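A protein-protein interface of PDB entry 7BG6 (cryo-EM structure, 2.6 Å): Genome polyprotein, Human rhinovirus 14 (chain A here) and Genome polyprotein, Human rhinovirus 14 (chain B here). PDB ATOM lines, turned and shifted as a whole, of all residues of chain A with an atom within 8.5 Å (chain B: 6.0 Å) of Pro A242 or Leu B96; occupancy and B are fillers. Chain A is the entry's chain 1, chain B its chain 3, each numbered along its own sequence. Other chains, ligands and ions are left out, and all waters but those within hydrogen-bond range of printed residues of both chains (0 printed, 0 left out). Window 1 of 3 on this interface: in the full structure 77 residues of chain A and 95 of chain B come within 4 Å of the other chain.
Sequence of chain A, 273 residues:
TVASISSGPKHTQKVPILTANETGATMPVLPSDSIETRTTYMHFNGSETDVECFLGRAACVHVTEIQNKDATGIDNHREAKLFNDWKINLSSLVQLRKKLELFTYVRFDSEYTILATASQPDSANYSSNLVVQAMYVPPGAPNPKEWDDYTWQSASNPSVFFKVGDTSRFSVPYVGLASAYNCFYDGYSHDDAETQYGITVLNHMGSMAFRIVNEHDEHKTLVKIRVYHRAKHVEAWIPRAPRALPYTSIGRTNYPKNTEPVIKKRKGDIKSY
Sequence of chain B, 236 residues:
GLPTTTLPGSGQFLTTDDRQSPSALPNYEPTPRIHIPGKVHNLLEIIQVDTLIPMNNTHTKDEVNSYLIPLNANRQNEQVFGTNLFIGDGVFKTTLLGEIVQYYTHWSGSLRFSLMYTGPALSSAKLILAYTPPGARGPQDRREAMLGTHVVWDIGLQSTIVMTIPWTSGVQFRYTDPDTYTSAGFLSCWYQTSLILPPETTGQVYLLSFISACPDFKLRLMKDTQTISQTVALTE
The side-chain amino group (NZ) of Lys A98 is in salt-bridge range of the side-chain carboxylate (OE2) of Glu B99 (3.0 Å). OE2 of Glu B99 lies close to O of Arg A243, at 3.4 Å.
NZ of Lys A98 lies within hydrogen-bond range of O of Arg A243, 2.8 Å away. NE of Arg A243 sits at hydrogen-bond distance from O of Leu A245, 2.6 Å away.
Among the printed residues, pairs that only touch across the chains: Pro A239 with Ile B46, Pro A242 with Leu B96, Pro A242 with Glu B99 and Val A262 with Thr B94.
Printed residues of chain B within 4 Å of Lys A98: Glu B99 (3.0 Å). Glu A101 touches none of the printed residues of chain B. Of the printed residues of chain B, Pro A239 touches Ile B46. Of chain B, only Leu B96 and Glu B99 come within 4 Å of Pro A242. Of the printed residues of chain B, Val A262 touches Thr B94 (3.5 Å). Phe B92 touches none of the printed residues of chain A. Printed residues of chain A within 4 Å of Thr B94: Val A262 (3.5 Å). Leu B96 touches one residue of chain A. Of the printed residues of chain A, Glu B99 touches Lys A98, Pro A242 and Arg A243. The nearest residue of chain B that does not touch Pro A242 is Thr B95 (5.1 Å). The nearest residue of chain A that does not touch Leu B96 is Arg A240 (4.2 Å). The nearest printed residue of chain B that does not touch Arg A243 is Thr B94 (7.0 Å).
Hydrophobic or aromatic side chains of chain A that line the printed part of chain B: Pro A239 and Pro A242. Of the 14 printed residues of chain B, 4 touch a printed residue of chain A. Printed residues of chain B that touch a printed residue of chain A: Ile B46, Thr B94, Leu B96 and Glu B99. Along chain B the printed residues that touch a printed residue of chain A span positions 46 to 99. Among the printed residues, Asp or Glu carboxylates within 4 Å of a Lys or Arg side-chain nitrogen of the other chain: Lys A98 with Glu B99 (3.0 Å).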
ATOM      1  N   LYS A  98     -19.692  -6.801  23.843  1.00  0.00           N
ATOM      2  CA  LYS A  98     -20.002  -8.132  23.344  1.00  0.00           C
ATOM      3  C   LYS A  98     -20.187  -9.103  24.511  1.00  0.00           C
ATOM      4  O   LYS A  98     -21.061  -9.967  24.460  1.00  0.00           O
ATOM      5  CB  LYS A  98     -18.921  -8.614  22.371  1.00  0.00           C
ATOM      6  CG  LYS A  98     -19.157  -9.994  21.771  1.00  0.00           C
ATOM      7  CD  LYS A  98     -18.266 -10.314  20.592  1.00  0.00           C
ATOM      8  CE  LYS A  98     -18.410 -11.748  20.130  1.00  0.00           C
ATOM      9  NZ  LYS A  98     -17.988 -11.913  18.719  1.00  0.00           N
ATOM     10  N   LYS A  99     -19.361  -8.944  25.552  1.00  0.00           N
ATOM     11  CA  LYS A  99     -19.399  -9.806  26.723  1.00  0.00           C
ATOM     12  C   LYS A  99     -20.727  -9.638  27.457  1.00  0.00           C
ATOM     13  O   LYS A  99     -21.363 -10.627  27.817  1.00  0.00           O
ATOM     14  CB  LYS A  99     -18.222  -9.514  27.661  1.00  0.00           C
ATOM     15  CG  LYS A  99     -16.870 -10.034  27.197  1.00  0.00           C
ATOM     16  CD  LYS A  99     -15.920 -10.366  28.331  1.00  0.00           C
ATOM     17  CE  LYS A  99     -15.409  -9.149  29.073  1.00  0.00           C
ATOM     18  NZ  LYS A  99     -14.528  -9.526  30.203  1.00  0.00           N
ATOM     19  N   GLU A 101     -23.419  -8.401  26.201  1.00  0.00           N
ATOM     20  CA  GLU A 101     -24.512  -8.641  25.273  1.00  0.00           C
ATOM     21  C   GLU A 101     -24.631 -10.128  24.942  1.00  0.00           C
ATOM     22  O   GLU A 101     -25.393 -10.504  24.052  1.00  0.00           O
ATOM     23  CB  GLU A 101     -24.350  -7.790  24.011  1.00  0.00           C
ATOM     24  CG  GLU A 101     -24.713  -6.331  24.222  1.00  0.00           C
ATOM     25  CD  GLU A 101     -24.823  -5.498  22.956  1.00  0.00           C
ATOM     26  OE1 GLU A 101     -25.061  -4.281  23.074  1.00  0.00           O
ATOM     27  OE2 GLU A 101     -24.681  -6.069  21.855  1.00  0.00           O
ATOM     28  N   LEU A 102     -23.879 -10.966  25.665  1.00  0.00           N
ATOM     29  CA  LEU A 102     -24.125 -12.398  25.655  1.00  0.00           C
ATOM     30  C   LEU A 102     -25.393 -12.676  26.461  1.00  0.00           C
ATOM     31  O   LEU A 102     -25.939 -13.774  26.402  1.00  0.00           O
ATOM     32  CB  LEU A 102     -22.923 -13.141  26.251  1.00  0.00           C
ATOM     33  CG  LEU A 102     -21.663 -13.204  25.387  1.00  0.00           C
ATOM     34  CD1 LEU A 102     -20.689 -14.232  25.938  1.00  0.00           C
ATOM     35  CD2 LEU A 102     -21.999 -13.530  23.939  1.00  0.00           C
ATOM     36  N   PHE A 103     -25.843 -11.656  27.202  1.00  0.00           N
ATOM     37  CA  PHE A 103     -26.992 -11.757  28.085  1.00  0.00           C
ATOM     38  C   PHE A 103     -27.956 -10.604  27.813  1.00  0.00           C
ATOM     39  O   PHE A 103     -27.575  -9.594  27.224  1.00  0.00           O
ATOM     40  CB  PHE A 103     -26.540 -11.764  29.549  1.00  0.00           C
ATOM     41  CG  PHE A 103     -25.394 -12.695  29.852  1.00  0.00           C
ATOM     42  CD1 PHE A 103     -24.084 -12.239  29.833  1.00  0.00           C
ATOM     43  CD2 PHE A 103     -25.622 -14.031  30.150  1.00  0.00           C
ATOM     44  CE1 PHE A 103     -23.028 -13.095  30.106  1.00  0.00           C
ATOM     45  CE2 PHE A 103     -24.565 -14.886  30.424  1.00  0.00           C
ATOM     46  CZ  PHE A 103     -23.270 -14.418  30.402  1.00  0.00           C
ATOM     47  N   PHE A 184     -30.575  -5.095  26.157  1.00  0.00           N
ATOM     48  CA  PHE A 184     -31.450  -4.984  25.003  1.00  0.00           C
ATOM     49  C   PHE A 184     -32.846  -4.586  25.469  1.00  0.00           C
ATOM     50  O   PHE A 184     -33.330  -5.073  26.489  1.00  0.00           O
ATOM     51  CB  PHE A 184     -31.491  -6.303  24.227  1.00  0.00           C
ATOM     52  CG  PHE A 184     -30.165  -6.722  23.647  1.00  0.00           C
ATOM     53  CD1 PHE A 184     -29.266  -7.465  24.396  1.00  0.00           C
ATOM     54  CD2 PHE A 184     -29.811  -6.364  22.355  1.00  0.00           C
ATOM     55  CE1 PHE A 184     -28.041  -7.842  23.865  1.00  0.00           C
ATOM     56  CE2 PHE A 184     -28.587  -6.746  21.824  1.00  0.00           C
ATOM     57  CZ  PHE A 184     -27.707  -7.486  22.578  1.00  0.00           C
ATOM     58  N   PRO A 239     -29.311 -15.910  28.146  1.00  0.00           N
ATOM     59  CA  PRO A 239     -28.154 -15.906  27.250  1.00  0.00           C
ATOM     60  C   PRO A 239     -28.619 -15.703  25.811  1.00  0.00           C
ATOM     61  O   PRO A 239     -29.694 -16.163  25.431  1.00  0.00           O
ATOM     62  CB  PRO A 239     -27.540 -17.301  27.434  1.00  0.00           C
ATOM     63  CG  PRO A 239     -28.696 -18.158  27.902  1.00  0.00           C
ATOM     64  CD  PRO A 239     -29.555 -17.233  28.740  1.00  0.00           C
ATOM     65  N   ARG A 240     -27.796 -15.002  25.026  1.00  0.00           N
ATOM     66  CA  ARG A 240     -28.182 -14.585  23.690  1.00  0.00           C
ATOM     67  C   ARG A 240     -27.176 -15.111  22.672  1.00  0.00           C
ATOM     68  O   ARG A 240     -26.125 -15.634  23.038  1.00  0.00           O
ATOM     69  CB  ARG A 240     -28.241 -13.057  23.608  1.00  0.00           C
ATOM     70  CG  ARG A 240     -29.187 -12.416  24.612  1.00  0.00           C
ATOM     71  CD  ARG A 240     -29.259 -10.913  24.434  1.00  0.00           C
ATOM     72  NE  ARG A 240     -29.917 -10.518  23.195  1.00  0.00           N
ATOM     73  CZ  ARG A 240     -31.232 -10.405  23.035  1.00  0.00           C
ATOM     74  NH1 ARG A 240     -32.052 -10.662  24.040  1.00  0.00           N
ATOM     75  NH2 ARG A 240     -31.724 -10.037  21.865  1.00  0.00           N
ATOM     76  N   ALA A 241     -27.535 -14.969  21.392  1.00  0.00           N
ATOM     77  CA  ALA A 241     -26.616 -15.202  20.293  1.00  0.00           C
ATOM     78  C   ALA A 241     -25.510 -14.151  20.350  1.00  0.00           C
ATOM     79  O   ALA A 241     -25.796 -12.961  20.476  1.00  0.00           O
ATOM     80  CB  ALA A 241     -27.363 -15.153  18.984  1.00  0.00           C
ATOM     81  N   PRO A 242     -24.220 -14.559  20.300  1.00  0.00           N
ATOM     82  CA  PRO A 242     -23.106 -13.610  20.342  1.00  0.00           C
ATOM     83  C   PRO A 242     -23.147 -12.638  19.165  1.00  0.00           C
ATOM     84  O   PRO A 242     -23.606 -12.991  18.080  1.00  0.00           O
ATOM     85  CB  PRO A 242     -21.859 -14.501  20.224  1.00  0.00           C
ATOM     86  CG  PRO A 242     -22.326 -15.863  20.686  1.00  0.00           C
ATOM     87  CD  PRO A 242     -23.765 -15.956  20.224  1.00  0.00           C
ATOM     88  N   ARG A 243     -22.667 -11.414  19.411  1.00  0.00           N
ATOM     89  CA  ARG A 243     -22.558 -10.396  18.379  1.00  0.00           C
ATOM     90  C   ARG A 243     -21.588 -10.883  17.305  1.00  0.00           C
ATOM     91  O   ARG A 243     -20.509 -11.381  17.620  1.00  0.00           O
ATOM     92  CB  ARG A 243     -22.093  -9.071  18.990  1.00  0.00           C
ATOM     93  CG  ARG A 243     -22.023  -7.916  18.000  1.00  0.00           C
ATOM     94  CD  ARG A 243     -23.390  -7.420  17.568  1.00  0.00           C
ATOM     95  NE  ARG A 243     -23.291  -6.358  16.576  1.00  0.00           N
ATOM     96  CZ  ARG A 243     -24.294  -5.576  16.192  1.00  0.00           C
ATOM     97  NH1 ARG A 243     -25.497  -5.723  16.722  1.00  0.00           N
ATOM     98  NH2 ARG A 243     -24.089  -4.642  15.281  1.00  0.00           N
ATOM     99  N   ALA A 244     -21.994 -10.735  16.040  1.00  0.00           N
ATOM    100  CA  ALA A 244     -21.212 -11.219  14.914  1.00  0.00           C
ATOM    101  C   ALA A 244     -20.684 -10.045  14.096  1.00  0.00           C
ATOM    102  O   ALA A 244     -19.503 -10.006  13.755  1.00  0.00           O
ATOM    103  CB  ALA A 244     -22.048 -12.152  14.074  1.00  0.00           C
ATOM    104  N   LEU A 245     -21.575  -9.095  13.789  1.00  0.00           N
ATOM    105  CA  LEU A 245     -21.231  -7.933  12.986  1.00  0.00           C
ATOM    106  C   LEU A 245     -20.806  -6.788  13.903  1.00  0.00           C
ATOM    107  O   LEU A 245     -21.198  -6.752  15.068  1.00  0.00           O
ATOM    108  CB  LEU A 245     -22.441  -7.542  12.131  1.00  0.00           C
ATOM    109  CG  LEU A 245     -22.878  -8.570  11.087  1.00  0.00           C
ATOM    110  CD1 LEU A 245     -24.114  -8.089  10.352  1.00  0.00           C
ATOM    111  CD2 LEU A 245     -21.761  -8.861  10.096  1.00  0.00           C
ATOM    112  N   TYR A 247     -20.508  -2.927  15.609  1.00  0.00           N
ATOM    113  CA  TYR A 247     -21.505  -1.973  16.068  1.00  0.00           C
ATOM    114  C   TYR A 247     -21.357  -0.662  15.301  1.00  0.00           C
ATOM    115  O   TYR A 247     -20.361  -0.448  14.613  1.00  0.00           O
ATOM    116  CB  TYR A 247     -21.366  -1.733  17.574  1.00  0.00           C
ATOM    117  CG  TYR A 247     -21.598  -2.942  18.444  1.00  0.00           C
ATOM    118  CD1 TYR A 247     -20.536  -3.629  19.011  1.00  0.00           C
ATOM    119  CD2 TYR A 247     -22.881  -3.396  18.712  1.00  0.00           C
ATOM    120  CE1 TYR A 247     -20.741  -4.736  19.819  1.00  0.00           C
ATOM    121  CE2 TYR A 247     -23.103  -4.501  19.517  1.00  0.00           C
ATOM    122  CZ  TYR A 247     -22.029  -5.174  20.073  1.00  0.00           C
ATOM    123  OH  TYR A 247     -22.235  -6.266  20.867  1.00  0.00           O
ATOM    124  N   VAL A 262     -18.708 -12.705   7.912  1.00  0.00           N
ATOM    125  CA  VAL A 262     -18.039 -13.059   9.155  1.00  0.00           C
ATOM    126  C   VAL A 262     -17.802 -14.568   9.215  1.00  0.00           C
ATOM    127  O   VAL A 262     -16.943 -15.026   9.966  1.00  0.00           O
ATOM    128  CB  VAL A 262     -18.787 -12.533  10.399  1.00  0.00           C
ATOM    129  CG1 VAL A 262     -18.863 -11.015  10.417  1.00  0.00           C
ATOM    130  CG2 VAL A 262     -20.171 -13.146  10.557  1.00  0.00           C
ATOM    131  N   ILE B  46     -24.254 -22.775  29.241  1.00  0.00           N
ATOM    132  CA  ILE B  46     -24.843 -22.368  27.975  1.00  0.00           C
ATOM    133  C   ILE B  46     -24.047 -22.951  26.808  1.00  0.00           C
ATOM    134  O   ILE B  46     -24.591 -23.120  25.719  1.00  0.00           O
ATOM    135  CB  ILE B  46     -24.988 -20.832  27.889  1.00  0.00           C
ATOM    136  CG1 ILE B  46     -23.634 -20.113  27.908  1.00  0.00           C
ATOM    137  CG2 ILE B  46     -25.916 -20.322  28.982  1.00  0.00           C
ATOM    138  CD1 ILE B  46     -23.696 -18.657  27.500  1.00  0.00           C
ATOM    139  N   ILE B  47     -22.768 -23.264  27.047  1.00  0.00           N
ATOM    140  CA  ILE B  47     -21.903 -23.807  26.008  1.00  0.00           C
ATOM    141  C   ILE B  47     -22.292 -25.258  25.723  1.00  0.00           C
ATOM    142  O   ILE B  47     -21.845 -25.840  24.736  1.00  0.00           O
ATOM    143  CB  ILE B  47     -20.409 -23.650  26.371  1.00  0.00           C
ATOM    144  CG1 ILE B  47     -19.518 -23.703  25.125  1.00  0.00           C
ATOM    145  CG2 ILE B  47     -19.986 -24.666  27.425  1.00  0.00           C
ATOM    146  CD1 ILE B  47     -18.044 -23.499  25.394  1.00  0.00           C
ATOM    147  N   VAL B  49     -25.257 -26.034  25.041  1.00  0.00           N
ATOM    148  CA  VAL B  49     -26.402 -25.910  24.153  1.00  0.00           C
ATOM    149  C   VAL B  49     -25.920 -26.026  22.708  1.00  0.00           C
ATOM    150  O   VAL B  49     -24.923 -25.414  22.330  1.00  0.00           O
ATOM    151  CB  VAL B  49     -27.178 -24.600  24.399  1.00  0.00           C
ATOM    152  CG1 VAL B  49     -28.303 -24.394  23.394  1.00  0.00           C
ATOM    153  CG2 VAL B  49     -27.718 -24.521  25.819  1.00  0.00           C
ATOM    154  N   THR B  51     -25.657 -25.393  18.862  1.00  0.00           N
ATOM    155  CA  THR B  51     -25.800 -24.301  17.911  1.00  0.00           C
ATOM    156  C   THR B  51     -25.360 -24.789  16.535  1.00  0.00           C
ATOM    157  O   THR B  51     -24.486 -25.649  16.430  1.00  0.00           O
ATOM    158  CB  THR B  51     -25.013 -23.057  18.344  1.00  0.00           C
ATOM    159  OG1 THR B  51     -23.674 -23.445  18.655  1.00  0.00           O
ATOM    160  CG2 THR B  51     -25.635 -22.342  19.524  1.00  0.00           C
ATOM    161  N   PHE B  92     -16.237 -23.361  13.105  1.00  0.00           N
ATOM    162  CA  PHE B  92     -16.670 -23.345  14.494  1.00  0.00           C
ATOM    163  C   PHE B  92     -16.571 -21.941  15.086  1.00  0.00           C
ATOM    164  O   PHE B  92     -17.157 -21.675  16.133  1.00  0.00           O
ATOM    165  CB  PHE B  92     -15.854 -24.338  15.324  1.00  0.00           C
ATOM    166  CG  PHE B  92     -15.999 -25.782  14.915  1.00  0.00           C
ATOM    167  CD1 PHE B  92     -14.988 -26.429  14.223  1.00  0.00           C
ATOM    168  CD2 PHE B  92     -17.149 -26.494  15.223  1.00  0.00           C
ATOM    169  CE1 PHE B  92     -15.122 -27.758  13.846  1.00  0.00           C
ATOM    170  CE2 PHE B  92     -17.284 -27.822  14.845  1.00  0.00           C
ATOM    171  CZ  PHE B  92     -16.270 -28.451  14.158  1.00  0.00           C
ATOM    172  N   THR B  94     -17.793 -19.089  14.516  1.00  0.00           N
ATOM    173  CA  THR B  94     -18.958 -18.223  14.607  1.00  0.00           C
ATOM    174  C   THR B  94     -20.043 -18.840  15.490  1.00  0.00           C
ATOM    175  O   THR B  94     -21.021 -18.170  15.821  1.00  0.00           O
ATOM    176  CB  THR B  94     -19.479 -17.857  13.210  1.00  0.00           C
ATOM    177  OG1 THR B  94     -19.699 -19.062  12.478  1.00  0.00           O
ATOM    178  CG2 THR B  94     -18.533 -16.957  12.443  1.00  0.00           C
ATOM    179  N   THR B  95     -19.863 -20.112  15.868  1.00  0.00           N
ATOM    180  CA  THR B  95     -20.810 -20.806  16.730  1.00  0.00           C
ATOM    181  C   THR B  95     -20.672 -20.283  18.159  1.00  0.00           C
ATOM    182  O   THR B  95     -19.663 -19.670  18.500  1.00  0.00           O
ATOM    183  CB  THR B  95     -20.617 -22.328  16.676  1.00  0.00           C
ATOM    184  OG1 THR B  95     -19.380 -22.659  17.308  1.00  0.00           O
ATOM    185  CG2 THR B  95     -20.649 -22.888  15.270  1.00  0.00           C
ATOM    186  N   LEU B  96     -21.694 -20.543  18.985  1.00  0.00           N
ATOM    187  CA  LEU B  96     -21.689 -20.138  20.383  1.00  0.00           C
ATOM    188  C   LEU B  96     -20.509 -20.789  21.102  1.00  0.00           C
ATOM    189  O   LEU B  96     -19.848 -20.143  21.911  1.00  0.00           O
ATOM    190  CB  LEU B  96     -23.023 -20.528  21.032  1.00  0.00           C
ATOM    191  CG  LEU B  96     -23.149 -20.247  22.530  1.00  0.00           C
ATOM    192  CD1 LEU B  96     -23.303 -18.758  22.801  1.00  0.00           C
ATOM    193  CD2 LEU B  96     -24.319 -21.013  23.123  1.00  0.00           C
ATOM    194  N   LEU B  97     -20.259 -22.068  20.790  1.00  0.00           N
ATOM    195  CA  LEU B  97     -19.129 -22.792  21.350  1.00  0.00           C
ATOM    196  C   LEU B  97     -17.837 -22.073  20.972  1.00  0.00           C
ATOM    197  O   LEU B  97     -17.018 -21.785  21.839  1.00  0.00           O
ATOM    198  CB  LEU B  97     -19.143 -24.238  20.840  1.00  0.00           C
ATOM    199  CG  LEU B  97     -18.145 -25.184  21.512  1.00  0.00           C
ATOM    200  CD1 LEU B  97     -18.737 -26.575  21.669  1.00  0.00           C
ATOM    201  CD2 LEU B  97     -16.836 -25.246  20.741  1.00  0.00           C
ATOM    202  N   GLY B  98     -17.684 -21.772  19.676  1.00  0.00           N
ATOM    203  CA  GLY B  98     -16.506 -21.096  19.159  1.00  0.00           C
ATOM    204  C   GLY B  98     -16.315 -19.708  19.767  1.00  0.00           C
ATOM    205  O   GLY B  98     -15.194 -19.325  20.095  1.00  0.00           O
ATOM    206  N   GLU B  99     -17.425 -18.975  19.919  1.00  0.00           N
ATOM    207  CA  GLU B  99     -17.411 -17.604  20.406  1.00  0.00           C
ATOM    208  C   GLU B  99     -16.983 -17.564  21.872  1.00  0.00           C
ATOM    209  O   GLU B  99     -16.181 -16.717  22.257  1.00  0.00           O
ATOM    210  CB  GLU B  99     -18.775 -16.938  20.203  1.00  0.00           C
ATOM    211  CG  GLU B  99     -19.062 -16.552  18.760  1.00  0.00           C
ATOM    212  CD  GLU B  99     -18.443 -15.248  18.283  1.00  0.00           C
ATOM    213  OE1 GLU B  99     -17.258 -15.008  18.587  1.00  0.00           O
ATOM    214  OE2 GLU B  99     -19.151 -14.474  17.608  1.00  0.00           O
ATOM    215  N   ILE B 100     -17.531 -18.485  22.678  1.00  0.00           N
ATOM    216  CA  ILE B 100     -17.205 -18.577  24.093  1.00  0.00           C
ATOM    217  C   ILE B 100     -15.775 -19.094  24.244  1.00  0.00           C
ATOM    218  O   ILE B 100     -15.032 -18.626  25.104  1.00  0.00           O
ATOM    219  CB  ILE B 100     -18.230 -19.451  24.850  1.00  0.00           C
ATOM    220  CG1 ILE B 100     -19.602 -18.776  24.926  1.00  0.00           C
ATOM    221  CG2 ILE B 100     -17.714 -19.828  26.232  1.00  0.00           C
ATOM    222  CD1 ILE B 100     -20.709 -19.675  25.434  1.00  0.00           C
ATOM    223  N   VAL B 101     -15.405 -20.051  23.383  1.00  0.00           N
ATOM    224  CA  VAL B 101     -14.099 -20.691  23.409  1.00  0.00           C
ATOM    225  C   VAL B 101     -13.005 -19.656  23.145  1.00  0.00           C
ATOM    226  O   VAL B 101     -11.920 -19.748  23.715  1.00  0.00           O
ATOM    227  CB  VAL B 101     -14.048 -21.885  22.431  1.00  0.00           C
ATOM    228  CG1 VAL B 101     -12.700 -22.056  21.748  1.00  0.00           C
ATOM    229  CG2 VAL B 101     -14.484 -23.180  23.101  1.00  0.00           C
ATOM    230  N   ILE B 211     -23.007 -28.160  17.134  1.00  0.00           N
ATOM    231  CA  ILE B 211     -21.875 -28.378  18.018  1.00  0.00           C
ATOM    232  C   ILE B 211     -22.249 -27.909  19.422  1.00  0.00           C
ATOM    233  O   ILE B 211     -22.833 -26.841  19.595  1.00  0.00           O
ATOM    234  CB  ILE B 211     -20.589 -27.705  17.482  1.00  0.00           C
ATOM    235  CG1 ILE B 211     -19.334 -28.168  18.232  1.00  0.00           C
ATOM    236  CG2 ILE B 211     -20.709 -26.188  17.462  1.00  0.00           C
ATOM    237  CD1 ILE B 211     -18.902 -29.583  17.909  1.00  0.00           C
